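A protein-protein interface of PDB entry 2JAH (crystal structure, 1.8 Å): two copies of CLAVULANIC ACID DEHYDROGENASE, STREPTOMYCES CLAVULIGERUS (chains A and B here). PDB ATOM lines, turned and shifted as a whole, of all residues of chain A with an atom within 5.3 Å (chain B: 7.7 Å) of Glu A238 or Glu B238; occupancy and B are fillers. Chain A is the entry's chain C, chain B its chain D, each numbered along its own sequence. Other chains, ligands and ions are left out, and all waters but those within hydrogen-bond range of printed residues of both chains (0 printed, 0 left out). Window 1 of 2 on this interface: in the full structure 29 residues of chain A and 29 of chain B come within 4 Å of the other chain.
O of Glu A238 sits at hydrogen-bond distance from N of Phe B240 (2.9 Å). NH2 of Arg B146 sits close to NH2 of Arg A146 (3.5 Å). The backbone carbonyl oxygen of Glu B238 is in hydrogen-bond range of the backbone NH of Phe A240. The backbone NH of His A237 sits at hydrogen-bond distance from the backbone carbonyl oxygen of Phe B240 (2.8 Å). NH2 of Arg A146 lies within salt-bridge range of OE1 of Glu B238 (2.8 Å). The backbone carbonyl oxygen of Phe A240 sits at hydrogen-bond distance from the backbone NH of His B237, 2.8 Å away. OE1 of Glu A238 lies within salt-bridge range of NH2 of Arg B146, 2.8 Å away.
The guanidinium group (NH1) of Arg B146 lies within salt-bridge range of the side-chain carboxylate (OE2) of Glu B238 (3.4 Å). The backbone carbonyl oxygen (O) of Val B182 is in hydrogen-bond range of the backbone NH (N) of Ile B239 (3.1 Å). The backbone NH (N) of Val B182 sits at hydrogen-bond distance from the backbone carbonyl oxygen (O) of His B237. The side-chain carboxylate (OE2) of Glu A184 lies close to the side-chain carboxylate (OE2) of Glu A238 (2.5 Å). O of Glu A184 lies within hydrogen-bond range of N of Ile A241, 3.1 Å away. The backbone NH (N) of Glu A184 lies within hydrogen-bond range of the backbone carbonyl oxygen (O) of Ile A239, at 2.8 Å.
Ile B239 touches Val A236 (CG2 to CG1, 3.8 Å). Val A236 touches Ile B241 (CG2 to CD1, 3.9 Å). Glu A238 touches Glu B238 (O to O, 3.7 Å). Ile B239 touches Glu A238. Val B236 touches Ile A239 (CG1 to CG2, 3.9 Å). Glu B238 touches Ile A239. Thr B235 touches Phe A240 (O to O, 3.8 Å). O of Phe A240 touches C of Val B236, 3.5 Å away. Thr B235 touches Ile A241. Val B236 touches Ile A241.
Glu A238 touches four residues of chain B. Of chain A, only Arg A146 (2.8 Å), Glu A238 (3.7 Å), Ile A239 (3.4 Å) and Phe A240 (2.8 Å) come within 4 Å of Glu B238. Printed residues of chain A within 4 Å of Ile B241: Val A236 (3.9 Å). Of the printed residues of chain B, Phe A240 touches Thr B235 (3.8 Å), Val B236 (3.5 Å), His B237 (2.8 Å) and Glu B238 (2.8 Å). Glu B184 touches none of the printed residues of chain A. Glu B167 touches none of the printed residues of chain A. The nearest printed residue of chain A that does not touch Glu B238 is Ile A241 (5.3 Å). The nearest printed residue of chain A that does not touch Val B236 is Glu A238 (6.9 Å).
Hydrophobic or aromatic side chains of chain A that line the printed part of chain B: Val A236, Ile A239, Phe A240 and Ile A241. Printed residues of chain B that touch a printed residue of chain A: Arg B146, Thr B235, Val B236, His B237, Glu B238, Ile B239, Phe B240 and Ile B241. Hydrophobic or aromatic side chains of chain B that line the printed part of chain A: Val B236, His B237, Ile B239, Phe B240 and Ile B241. Among the printed residues, 18 pairs touch across the chains.
Arg A146 touches its own counterpart, Arg B146. Arg A146 touches Glu B238, and with the chains exchanged Glu A238 touches Arg B146. Val A236 touches Ile B241, and with the chains exchanged Ile A241 touches Val B236. His A237 touches Phe B240, and with the chains exchanged Phe A240 touches His B237. Positions printed for both chains: 146, 163, 182, 184, 236, 237, 238, 239, 240 and 241.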
ATOM      1  N   ARG A 146       2.990   8.377 -15.430  1.00  0.00           N
ATOM      2  CA  ARG A 146       1.690   7.871 -14.940  1.00  0.00           C
ATOM      3  C   ARG A 146       1.561   6.351 -15.051  1.00  0.00           C
ATOM      4  O   ARG A 146       0.827   5.731 -14.283  1.00  0.00           O
ATOM      5  CB  ARG A 146       0.524   8.515 -15.725  1.00  0.00           C
ATOM      6  CG  ARG A 146       0.439  10.042 -15.699  1.00  0.00           C
ATOM      7  CD  ARG A 146       0.149  10.647 -14.291  1.00  0.00           C
ATOM      8  NE  ARG A 146      -1.073  10.103 -13.687  1.00  0.00           N
ATOM      9  CZ  ARG A 146      -2.309  10.445 -14.055  1.00  0.00           C
ATOM     10  NH1 ARG A 146      -2.507  11.368 -14.992  1.00  0.00           N
ATOM     11  NH2 ARG A 146      -3.353   9.880 -13.467  1.00  0.00           N
ATOM     12  N   ASN A 163       6.712  14.616 -11.849  1.00  0.00           N
ATOM     13  CA  ASN A 163       5.335  14.794 -11.359  1.00  0.00           C
ATOM     14  C   ASN A 163       5.274  15.090  -9.863  1.00  0.00           C
ATOM     15  O   ASN A 163       4.585  16.035  -9.440  1.00  0.00           O
ATOM     16  CB  ASN A 163       4.447  13.601 -11.731  1.00  0.00           C
ATOM     17  CG  ASN A 163       4.107  13.582 -13.218  1.00  0.00           C
ATOM     18  OD1 ASN A 163       4.727  14.273 -14.008  1.00  0.00           O
ATOM     19  ND2 ASN A 163       3.123  12.793 -13.587  1.00  0.00           N
ATOM     20  N   VAL A 182       1.297  20.446 -15.594  1.00  0.00           N
ATOM     21  CA  VAL A 182       2.049  19.249 -16.007  1.00  0.00           C
ATOM     22  C   VAL A 182       1.358  18.601 -17.192  1.00  0.00           C
ATOM     23  O   VAL A 182       0.173  18.228 -17.099  1.00  0.00           O
ATOM     24  CB  VAL A 182       2.190  18.216 -14.854  1.00  0.00           C
ATOM     25  CG1 VAL A 182       2.993  17.007 -15.311  1.00  0.00           C
ATOM     26  CG2 VAL A 182       2.854  18.863 -13.630  1.00  0.00           C
ATOM     27  N   GLU A 184       1.299  15.568 -19.959  1.00  0.00           N
ATOM     28  CA  GLU A 184       1.708  14.170 -20.010  1.00  0.00           C
ATOM     29  C   GLU A 184       1.315  13.574 -21.359  1.00  0.00           C
ATOM     30  O   GLU A 184       0.247  12.962 -21.483  1.00  0.00           O
ATOM     31  CB  GLU A 184       1.078  13.379 -18.859  1.00  0.00           C
ATOM     32  CG  GLU A 184       1.558  13.841 -17.489  1.00  0.00           C
ATOM     33  CD  GLU A 184       0.552  13.613 -16.366  1.00  0.00           C
ATOM     34  OE1 GLU A 184      -0.615  13.206 -16.620  1.00  0.00           O
ATOM     35  OE2 GLU A 184       0.953  13.840 -15.202  1.00  0.00           O
ATOM     36  N   VAL A 236      -4.460  24.410 -14.505  1.00  0.00           N
ATOM     37  CA  VAL A 236      -4.677  23.129 -15.164  1.00  0.00           C
ATOM     38  C   VAL A 236      -3.463  22.269 -14.818  1.00  0.00           C
ATOM     39  O   VAL A 236      -2.448  22.249 -15.536  1.00  0.00           O
ATOM     40  CB  VAL A 236      -4.907  23.294 -16.677  1.00  0.00           C
ATOM     41  CG1 VAL A 236      -5.228  21.946 -17.298  1.00  0.00           C
ATOM     42  CG2 VAL A 236      -6.057  24.276 -16.927  1.00  0.00           C
ATOM     43  N   HIS A 237      -3.542  21.594 -13.673  1.00  0.00           N
ATOM     44  CA  HIS A 237      -2.349  20.978 -13.136  1.00  0.00           C
ATOM     45  C   HIS A 237      -1.880  19.762 -13.930  1.00  0.00           C
ATOM     46  O   HIS A 237      -0.692  19.449 -13.926  1.00  0.00           O
ATOM     47  CB  HIS A 237      -2.499  20.607 -11.658  1.00  0.00           C
ATOM     48  CG  HIS A 237      -1.243  20.059 -11.056  1.00  0.00           C
ATOM     49  ND1 HIS A 237      -0.073  20.784 -10.998  1.00  0.00           N
ATOM     50  CD2 HIS A 237      -0.967  18.857 -10.492  1.00  0.00           C
ATOM     51  CE1 HIS A 237       0.870  20.054 -10.426  1.00  0.00           C
ATOM     52  NE2 HIS A 237       0.352  18.882 -10.104  1.00  0.00           N
ATOM     53  N   GLU A 238      -2.812  19.042 -14.548  1.00  0.00           N
ATOM     54  CA  GLU A 238      -2.448  17.870 -15.336  1.00  0.00           C
ATOM     55  C   GLU A 238      -3.288  17.754 -16.603  1.00  0.00           C
ATOM     56  O   GLU A 238      -4.510  17.858 -16.552  1.00  0.00           O
ATOM     57  CB  GLU A 238      -2.597  16.582 -14.518  1.00  0.00           C
ATOM     58  CG  GLU A 238      -1.347  16.138 -13.823  1.00  0.00           C
ATOM     59  CD  GLU A 238      -1.515  14.816 -13.060  1.00  0.00           C
ATOM     60  OE1 GLU A 238      -2.364  14.761 -12.155  1.00  0.00           O
ATOM     61  OE2 GLU A 238      -0.750  13.857 -13.330  1.00  0.00           O
ATOM     62  N   ILE A 239      -2.619  17.555 -17.737  1.00  0.00           N
ATOM     63  CA  ILE A 239      -3.307  17.142 -18.964  1.00  0.00           C
ATOM     64  C   ILE A 239      -2.630  15.871 -19.431  1.00  0.00           C
ATOM     65  O   ILE A 239      -1.429  15.882 -19.736  1.00  0.00           O
ATOM     66  CB  ILE A 239      -3.249  18.204 -20.091  1.00  0.00           C
ATOM     67  CG1 ILE A 239      -3.865  19.528 -19.621  1.00  0.00           C
ATOM     68  CG2 ILE A 239      -3.975  17.670 -21.349  1.00  0.00           C
ATOM     69  CD1 ILE A 239      -3.714  20.690 -20.612  1.00  0.00           C
ATOM     70  N   PHE A 240      -3.392  14.779 -19.435  1.00  0.00           N
ATOM     71  CA  PHE A 240      -2.910  13.459 -19.850  1.00  0.00           C
ATOM     72  C   PHE A 240      -3.541  13.177 -21.215  1.00  0.00           C
ATOM     73  O   PHE A 240      -4.743  12.917 -21.325  1.00  0.00           O
ATOM     74  CB  PHE A 240      -3.292  12.407 -18.771  1.00  0.00           C
ATOM     75  CG  PHE A 240      -2.724  11.021 -18.985  1.00  0.00           C
ATOM     76  CD1 PHE A 240      -1.688  10.768 -19.892  1.00  0.00           C
ATOM     77  CD2 PHE A 240      -3.208   9.961 -18.213  1.00  0.00           C
ATOM     78  CE1 PHE A 240      -1.173   9.476 -20.055  1.00  0.00           C
ATOM     79  CE2 PHE A 240      -2.706   8.673 -18.368  1.00  0.00           C
ATOM     80  CZ  PHE A 240      -1.684   8.426 -19.290  1.00  0.00           C
ATOM     81  N   ILE A 241      -2.723  13.294 -22.261  1.00  0.00           N
ATOM     82  CA  ILE A 241      -3.199  13.128 -23.626  1.00  0.00           C
ATOM     83  C   ILE A 241      -2.557  11.880 -24.246  1.00  0.00           C
ATOM     84  O   ILE A 241      -1.331  11.741 -24.247  1.00  0.00           O
ATOM     85  CB  ILE A 241      -2.998  14.459 -24.450  1.00  0.00           C
ATOM     86  CG1 ILE A 241      -3.521  14.345 -25.894  1.00  0.00           C
ATOM     87  CG2 ILE A 241      -1.565  14.999 -24.341  1.00  0.00           C
ATOM     88  CD1 ILE A 241      -3.608  15.725 -26.624  1.00  0.00           C
ATOM     89  N   SER B 141     -15.537  13.633 -13.442  1.00  0.00           N
ATOM     90  CA  SER B 141     -15.026  13.155 -12.163  1.00  0.00           C
ATOM     91  C   SER B 141     -14.804  14.372 -11.260  1.00  0.00           C
ATOM     92  O   SER B 141     -15.649  15.267 -11.215  1.00  0.00           O
ATOM     93  CB  SER B 141     -13.756  12.328 -12.376  1.00  0.00           C
ATOM     94  OG  SER B 141     -13.290  11.730 -11.164  1.00  0.00           O
ATOM     95  N   SER B 142     -13.683  14.410 -10.547  1.00  0.00           N
ATOM     96  CA  SER B 142     -13.449  15.444  -9.552  1.00  0.00           C
ATOM     97  C   SER B 142     -12.017  15.318  -9.073  1.00  0.00           C
ATOM     98  O   SER B 142     -11.403  14.265  -9.256  1.00  0.00           O
ATOM     99  CB  SER B 142     -14.388  15.196  -8.358  1.00  0.00           C
ATOM    100  OG  SER B 142     -14.068  16.006  -7.247  1.00  0.00           O
ATOM    101  N   GLY B 145     -11.574  12.257  -7.186  1.00  0.00           N
ATOM    102  CA  GLY B 145     -11.142  11.022  -7.835  1.00  0.00           C
ATOM    103  C   GLY B 145      -9.624  10.886  -7.894  1.00  0.00           C
ATOM    104  O   GLY B 145      -9.108   9.881  -8.393  1.00  0.00           O
ATOM    105  N   ARG B 146      -8.923  11.906  -7.395  1.00  0.00           N
ATOM    106  CA  ARG B 146      -7.448  11.951  -7.376  1.00  0.00           C
ATOM    107  C   ARG B 146      -6.847  12.139  -5.977  1.00  0.00           C
ATOM    108  O   ARG B 146      -5.729  11.665  -5.700  1.00  0.00           O
ATOM    109  CB  ARG B 146      -6.935  13.084  -8.289  1.00  0.00           C
ATOM    110  CG  ARG B 146      -7.413  13.005  -9.758  1.00  0.00           C
ATOM    111  CD  ARG B 146      -6.853  11.766 -10.506  1.00  0.00           C
ATOM    112  NE  ARG B 146      -5.396  11.700 -10.428  1.00  0.00           N
ATOM    113  CZ  ARG B 146      -4.582  12.433 -11.182  1.00  0.00           C
ATOM    114  NH1 ARG B 146      -5.093  13.262 -12.090  1.00  0.00           N
ATOM    115  NH2 ARG B 146      -3.270  12.326 -11.034  1.00  0.00           N
ATOM    116  N   ASN B 163     -13.122   6.905 -12.188  1.00  0.00           N
ATOM    117  CA  ASN B 163     -11.818   6.946 -12.856  1.00  0.00           C
ATOM    118  C   ASN B 163     -11.323   5.571 -13.301  1.00  0.00           C
ATOM    119  O   ASN B 163     -10.877   5.424 -14.444  1.00  0.00           O
ATOM    120  CB  ASN B 163     -10.762   7.682 -11.995  1.00  0.00           C
ATOM    121  CG  ASN B 163     -10.977   9.199 -11.989  1.00  0.00           C
ATOM    122  OD1 ASN B 163     -12.016   9.686 -12.409  1.00  0.00           O
ATOM    123  ND2 ASN B 163      -9.987   9.941 -11.525  1.00  0.00           N
ATOM    124  N   GLU B 167     -10.854   4.412 -17.109  1.00  0.00           N
ATOM    125  CA  GLU B 167      -9.588   3.921 -17.667  1.00  0.00           C
ATOM    126  C   GLU B 167      -9.768   2.543 -18.299  1.00  0.00           C
ATOM    127  O   GLU B 167      -9.237   2.268 -19.382  1.00  0.00           O
ATOM    128  CB  GLU B 167      -8.452   3.909 -16.626  1.00  0.00           C
ATOM    129  CG  GLU B 167      -7.244   3.033 -17.019  1.00  0.00           C
ATOM    130  CD  GLU B 167      -6.619   3.402 -18.384  1.00  0.00           C
ATOM    131  OE1 GLU B 167      -6.832   4.522 -18.904  1.00  0.00           O
ATOM    132  OE2 GLU B 167      -5.904   2.547 -18.947  1.00  0.00           O
ATOM    133  N   VAL B 180     -12.260   8.282 -24.571  1.00  0.00           N
ATOM    134  CA  VAL B 180     -12.691   8.392 -23.183  1.00  0.00           C
ATOM    135  C   VAL B 180     -11.932   9.523 -22.493  1.00  0.00           C
ATOM    136  O   VAL B 180     -10.706   9.467 -22.321  1.00  0.00           O
ATOM    137  CB  VAL B 180     -12.519   7.064 -22.413  1.00  0.00           C
ATOM    138  CG1 VAL B 180     -12.946   7.243 -20.950  1.00  0.00           C
ATOM    139  CG2 VAL B 180     -13.319   5.953 -23.077  1.00  0.00           C
ATOM    140  N   VAL B 181     -12.687  10.536 -22.091  1.00  0.00           N
ATOM    141  CA  VAL B 181     -12.151  11.776 -21.521  1.00  0.00           C
ATOM    142  C   VAL B 181     -12.663  11.895 -20.092  1.00  0.00           C
ATOM    143  O   VAL B 181     -13.878  11.753 -19.846  1.00  0.00           O
ATOM    144  CB  VAL B 181     -12.619  13.001 -22.364  1.00  0.00           C
ATOM    145  CG1 VAL B 181     -12.262  14.326 -21.690  1.00  0.00           C
ATOM    146  CG2 VAL B 181     -12.035  12.932 -23.770  1.00  0.00           C
ATOM    147  N   VAL B 182     -11.751  12.135 -19.151  1.00  0.00           N
ATOM    148  CA  VAL B 182     -12.126  12.304 -17.761  1.00  0.00           C
ATOM    149  C   VAL B 182     -11.736  13.699 -17.301  1.00  0.00           C
ATOM    150  O   VAL B 182     -10.568  14.088 -17.380  1.00  0.00           O
ATOM    151  CB  VAL B 182     -11.496  11.231 -16.820  1.00  0.00           C
ATOM    152  CG1 VAL B 182     -12.033  11.413 -15.420  1.00  0.00           C
ATOM    153  CG2 VAL B 182     -11.795   9.825 -17.316  1.00  0.00           C
ATOM    154  N   ILE B 183     -12.723  14.458 -16.831  1.00  0.00           N
ATOM    155  CA  ILE B 183     -12.468  15.818 -16.381  1.00  0.00           C
ATOM    156  C   ILE B 183     -12.510  15.815 -14.857  1.00  0.00           C
ATOM    157  O   ILE B 183     -13.425  15.251 -14.273  1.00  0.00           O
ATOM    158  CB  ILE B 183     -13.522  16.828 -16.939  1.00  0.00           C
ATOM    159  CG1 ILE B 183     -13.601  16.796 -18.478  1.00  0.00           C
ATOM    160  CG2 ILE B 183     -13.256  18.234 -16.403  1.00  0.00           C
ATOM    161  CD1 ILE B 183     -12.329  17.178 -19.221  1.00  0.00           C
ATOM    162  N   GLU B 184     -11.527  16.453 -14.229  1.00  0.00           N
ATOM    163  CA  GLU B 184     -11.362  16.424 -12.774  1.00  0.00           C
ATOM    164  C   GLU B 184     -11.275  17.832 -12.183  1.00  0.00           C
ATOM    165  O   GLU B 184     -10.183  18.359 -11.959  1.00  0.00           O
ATOM    166  CB  GLU B 184     -10.118  15.612 -12.409  1.00  0.00           C
ATOM    167  CG  GLU B 184     -10.280  14.154 -12.739  1.00  0.00           C
ATOM    168  CD  GLU B 184      -8.960  13.453 -12.978  1.00  0.00           C
ATOM    169  OE1 GLU B 184      -7.900  14.114 -12.936  1.00  0.00           O
ATOM    170  OE2 GLU B 184      -9.001  12.238 -13.236  1.00  0.00           O
ATOM    171  N   TYR B 226     -12.253  21.861 -25.083  1.00  0.00           N
ATOM    172  CA  TYR B 226     -10.896  21.555 -25.517  1.00  0.00           C
ATOM    173  C   TYR B 226     -10.729  20.054 -25.821  1.00  0.00           C
ATOM    174  O   TYR B 226     -10.208  19.688 -26.874  1.00  0.00           O
ATOM    175  CB  TYR B 226      -9.833  22.072 -24.510  1.00  0.00           C
ATOM    176  CG  TYR B 226      -8.510  21.358 -24.672  1.00  0.00           C
ATOM    177  CD1 TYR B 226      -7.702  21.559 -25.806  1.00  0.00           C
ATOM    178  CD2 TYR B 226      -8.079  20.452 -23.704  1.00  0.00           C
ATOM    179  CE1 TYR B 226      -6.503  20.852 -25.962  1.00  0.00           C
ATOM    180  CE2 TYR B 226      -6.893  19.755 -23.852  1.00  0.00           C
ATOM    181  CZ  TYR B 226      -6.116  19.957 -24.972  1.00  0.00           C
ATOM    182  OH  TYR B 226      -4.956  19.224 -25.072  1.00  0.00           O
ATOM    183  N   ALA B 227     -11.164  19.200 -24.895  1.00  0.00           N
ATOM    184  CA  ALA B 227     -11.017  17.754 -25.053  1.00  0.00           C
ATOM    185  C   ALA B 227     -11.773  17.198 -26.263  1.00  0.00           C
ATOM    186  O   ALA B 227     -11.253  16.348 -26.985  1.00  0.00           O
ATOM    187  CB  ALA B 227     -11.450  17.035 -23.780  1.00  0.00           C
ATOM    188  N   THR B 235      -6.676  11.446 -27.573  1.00  0.00           N
ATOM    189  CA  THR B 235      -7.631  11.288 -26.489  1.00  0.00           C
ATOM    190  C   THR B 235      -7.079  12.056 -25.290  1.00  0.00           C
ATOM    191  O   THR B 235      -6.060  11.675 -24.713  1.00  0.00           O
ATOM    192  CB  THR B 235      -7.866   9.800 -26.143  1.00  0.00           C
ATOM    193  OG1 THR B 235      -8.584   9.175 -27.216  1.00  0.00           O
ATOM    194  CG2 THR B 235      -8.687   9.641 -24.850  1.00  0.00           C
ATOM    195  N   VAL B 236      -7.743  13.149 -24.933  1.00  0.00           N
ATOM    196  CA  VAL B 236      -7.372  13.877 -23.716  1.00  0.00           C
ATOM    197  C   VAL B 236      -8.025  13.119 -22.574  1.00  0.00           C
ATOM    198  O   VAL B 236      -9.171  13.390 -22.205  1.00  0.00           O
ATOM    199  CB  VAL B 236      -7.775  15.380 -23.808  1.00  0.00           C
ATOM    200  CG1 VAL B 236      -7.302  16.168 -22.587  1.00  0.00           C
ATOM    201  CG2 VAL B 236      -7.194  15.992 -25.071  1.00  0.00           C
ATOM    202  N   HIS B 237      -7.304  12.122 -22.052  1.00  0.00           N
ATOM    203  CA  HIS B 237      -7.886  11.193 -21.098  1.00  0.00           C
ATOM    204  C   HIS B 237      -8.146  11.794 -19.726  1.00  0.00           C
ATOM    205  O   HIS B 237      -9.072  11.377 -19.037  1.00  0.00           O
ATOM    206  CB  HIS B 237      -7.056   9.909 -20.948  1.00  0.00           C
ATOM    207  CG  HIS B 237      -7.707   8.882 -20.070  1.00  0.00           C
ATOM    208  ND1 HIS B 237      -8.970   8.383 -20.318  1.00  0.00           N
ATOM    209  CD2 HIS B 237      -7.279   8.267 -18.941  1.00  0.00           C
ATOM    210  CE1 HIS B 237      -9.292   7.511 -19.382  1.00  0.00           C
ATOM    211  NE2 HIS B 237      -8.283   7.427 -18.529  1.00  0.00           N
ATOM    212  N   GLU B 238      -7.320  12.747 -19.320  1.00  0.00           N
ATOM    213  CA  GLU B 238      -7.507  13.399 -18.026  1.00  0.00           C
ATOM    214  C   GLU B 238      -7.132  14.867 -18.122  1.00  0.00           C
ATOM    215  O   GLU B 238      -6.095  15.213 -18.683  1.00  0.00           O
ATOM    216  CB  GLU B 238      -6.671  12.729 -16.917  1.00  0.00           C
ATOM    217  CG  GLU B 238      -7.344  11.564 -16.188  1.00  0.00           C
ATOM    218  CD  GLU B 238      -6.490  10.981 -15.056  1.00  0.00           C
ATOM    219  OE1 GLU B 238      -5.376  10.479 -15.352  1.00  0.00           O
ATOM    220  OE2 GLU B 238      -6.951  11.006 -13.884  1.00  0.00           O
ATOM    221  N   ILE B 239      -7.991  15.718 -17.553  1.00  0.00           N
ATOM    222  CA  ILE B 239      -7.688  17.137 -17.324  1.00  0.00           C
ATOM    223  C   ILE B 239      -8.039  17.388 -15.870  1.00  0.00           C
ATOM    224  O   ILE B 239      -9.199  17.248 -15.465  1.00  0.00           O
ATOM    225  CB  ILE B 239      -8.542  18.086 -18.209  1.00  0.00           C
ATOM    226  CG1 ILE B 239      -8.383  17.740 -19.700  1.00  0.00           C
ATOM    227  CG2 ILE B 239      -8.183  19.570 -17.916  1.00  0.00           C
ATOM    228  CD1 ILE B 239      -9.169  18.638 -20.619  1.00  0.00           C
ATOM    229  N   PHE B 240      -7.021  17.738 -15.097  1.00  0.00           N
ATOM    230  CA  PHE B 240      -7.127  17.947 -13.665  1.00  0.00           C
ATOM    231  C   PHE B 240      -6.948  19.447 -13.503  1.00  0.00           C
ATOM    232  O   PHE B 240      -5.875  19.986 -13.774  1.00  0.00           O
ATOM    233  CB  PHE B 240      -6.018  17.140 -12.972  1.00  0.00           C
ATOM    234  CG  PHE B 240      -6.056  17.159 -11.469  1.00  0.00           C
ATOM    235  CD1 PHE B 240      -7.163  17.658 -10.755  1.00  0.00           C
ATOM    236  CD2 PHE B 240      -4.977  16.634 -10.755  1.00  0.00           C
ATOM    237  CE1 PHE B 240      -7.162  17.656  -9.353  1.00  0.00           C
ATOM    238  CE2 PHE B 240      -4.973  16.630  -9.361  1.00  0.00           C
ATOM    239  CZ  PHE B 240      -6.061  17.129  -8.658  1.00  0.00           C
ATOM    240  N   ILE B 241      -8.037  20.122 -13.134  1.00  0.00           N
ATOM    241  CA  ILE B 241      -8.065  21.581 -13.086  1.00  0.00           C
ATOM    242  C   ILE B 241      -8.408  22.042 -11.657  1.00  0.00           C
ATOM    243  O   ILE B 241      -9.444  21.663 -11.103  1.00  0.00           O
ATOM    244  CB  ILE B 241      -8.987  22.182 -14.214  1.00  0.00           C
ATOM    245  CG1 ILE B 241      -9.107  23.711 -14.090  1.00  0.00           C
ATOM    246  CG2 ILE B 241     -10.357  21.452 -14.286  1.00  0.00           C
ATOM    247  CD1 ILE B 241      -9.612  24.403 -15.405  1.00  0.00           C
ATOM    248  N   ARG B 242      -7.496  22.801 -11.057  1.00  0.00           N
ATOM    249  CA  ARG B 242      -7.577  23.165  -9.637  1.00  0.00           C
ATOM    250  C   ARG B 242      -7.693  24.684  -9.520  1.00  0.00           C
ATOM    251  O   ARG B 242      -7.208  25.410 -10.386  1.00  0.00           O
ATOM    252  CB  ARG B 242      -6.291  22.746  -8.888  1.00  0.00           C
ATOM    253  CG  ARG B 242      -5.998  21.270  -8.749  1.00  0.00           C
ATOM    254  CD  ARG B 242      -4.703  21.167  -7.984  1.00  0.00           C
ATOM    255  NE  ARG B 242      -4.369  19.839  -7.487  1.00  0.00           N
ATOM    256  CZ  ARG B 242      -4.529  19.439  -6.230  1.00  0.00           C
ATOM    257  NH1 ARG B 242      -5.051  20.247  -5.322  1.00  0.00           N
ATOM    258  NH2 ARG B 242      -4.170  18.213  -5.887  1.00  0.00           N
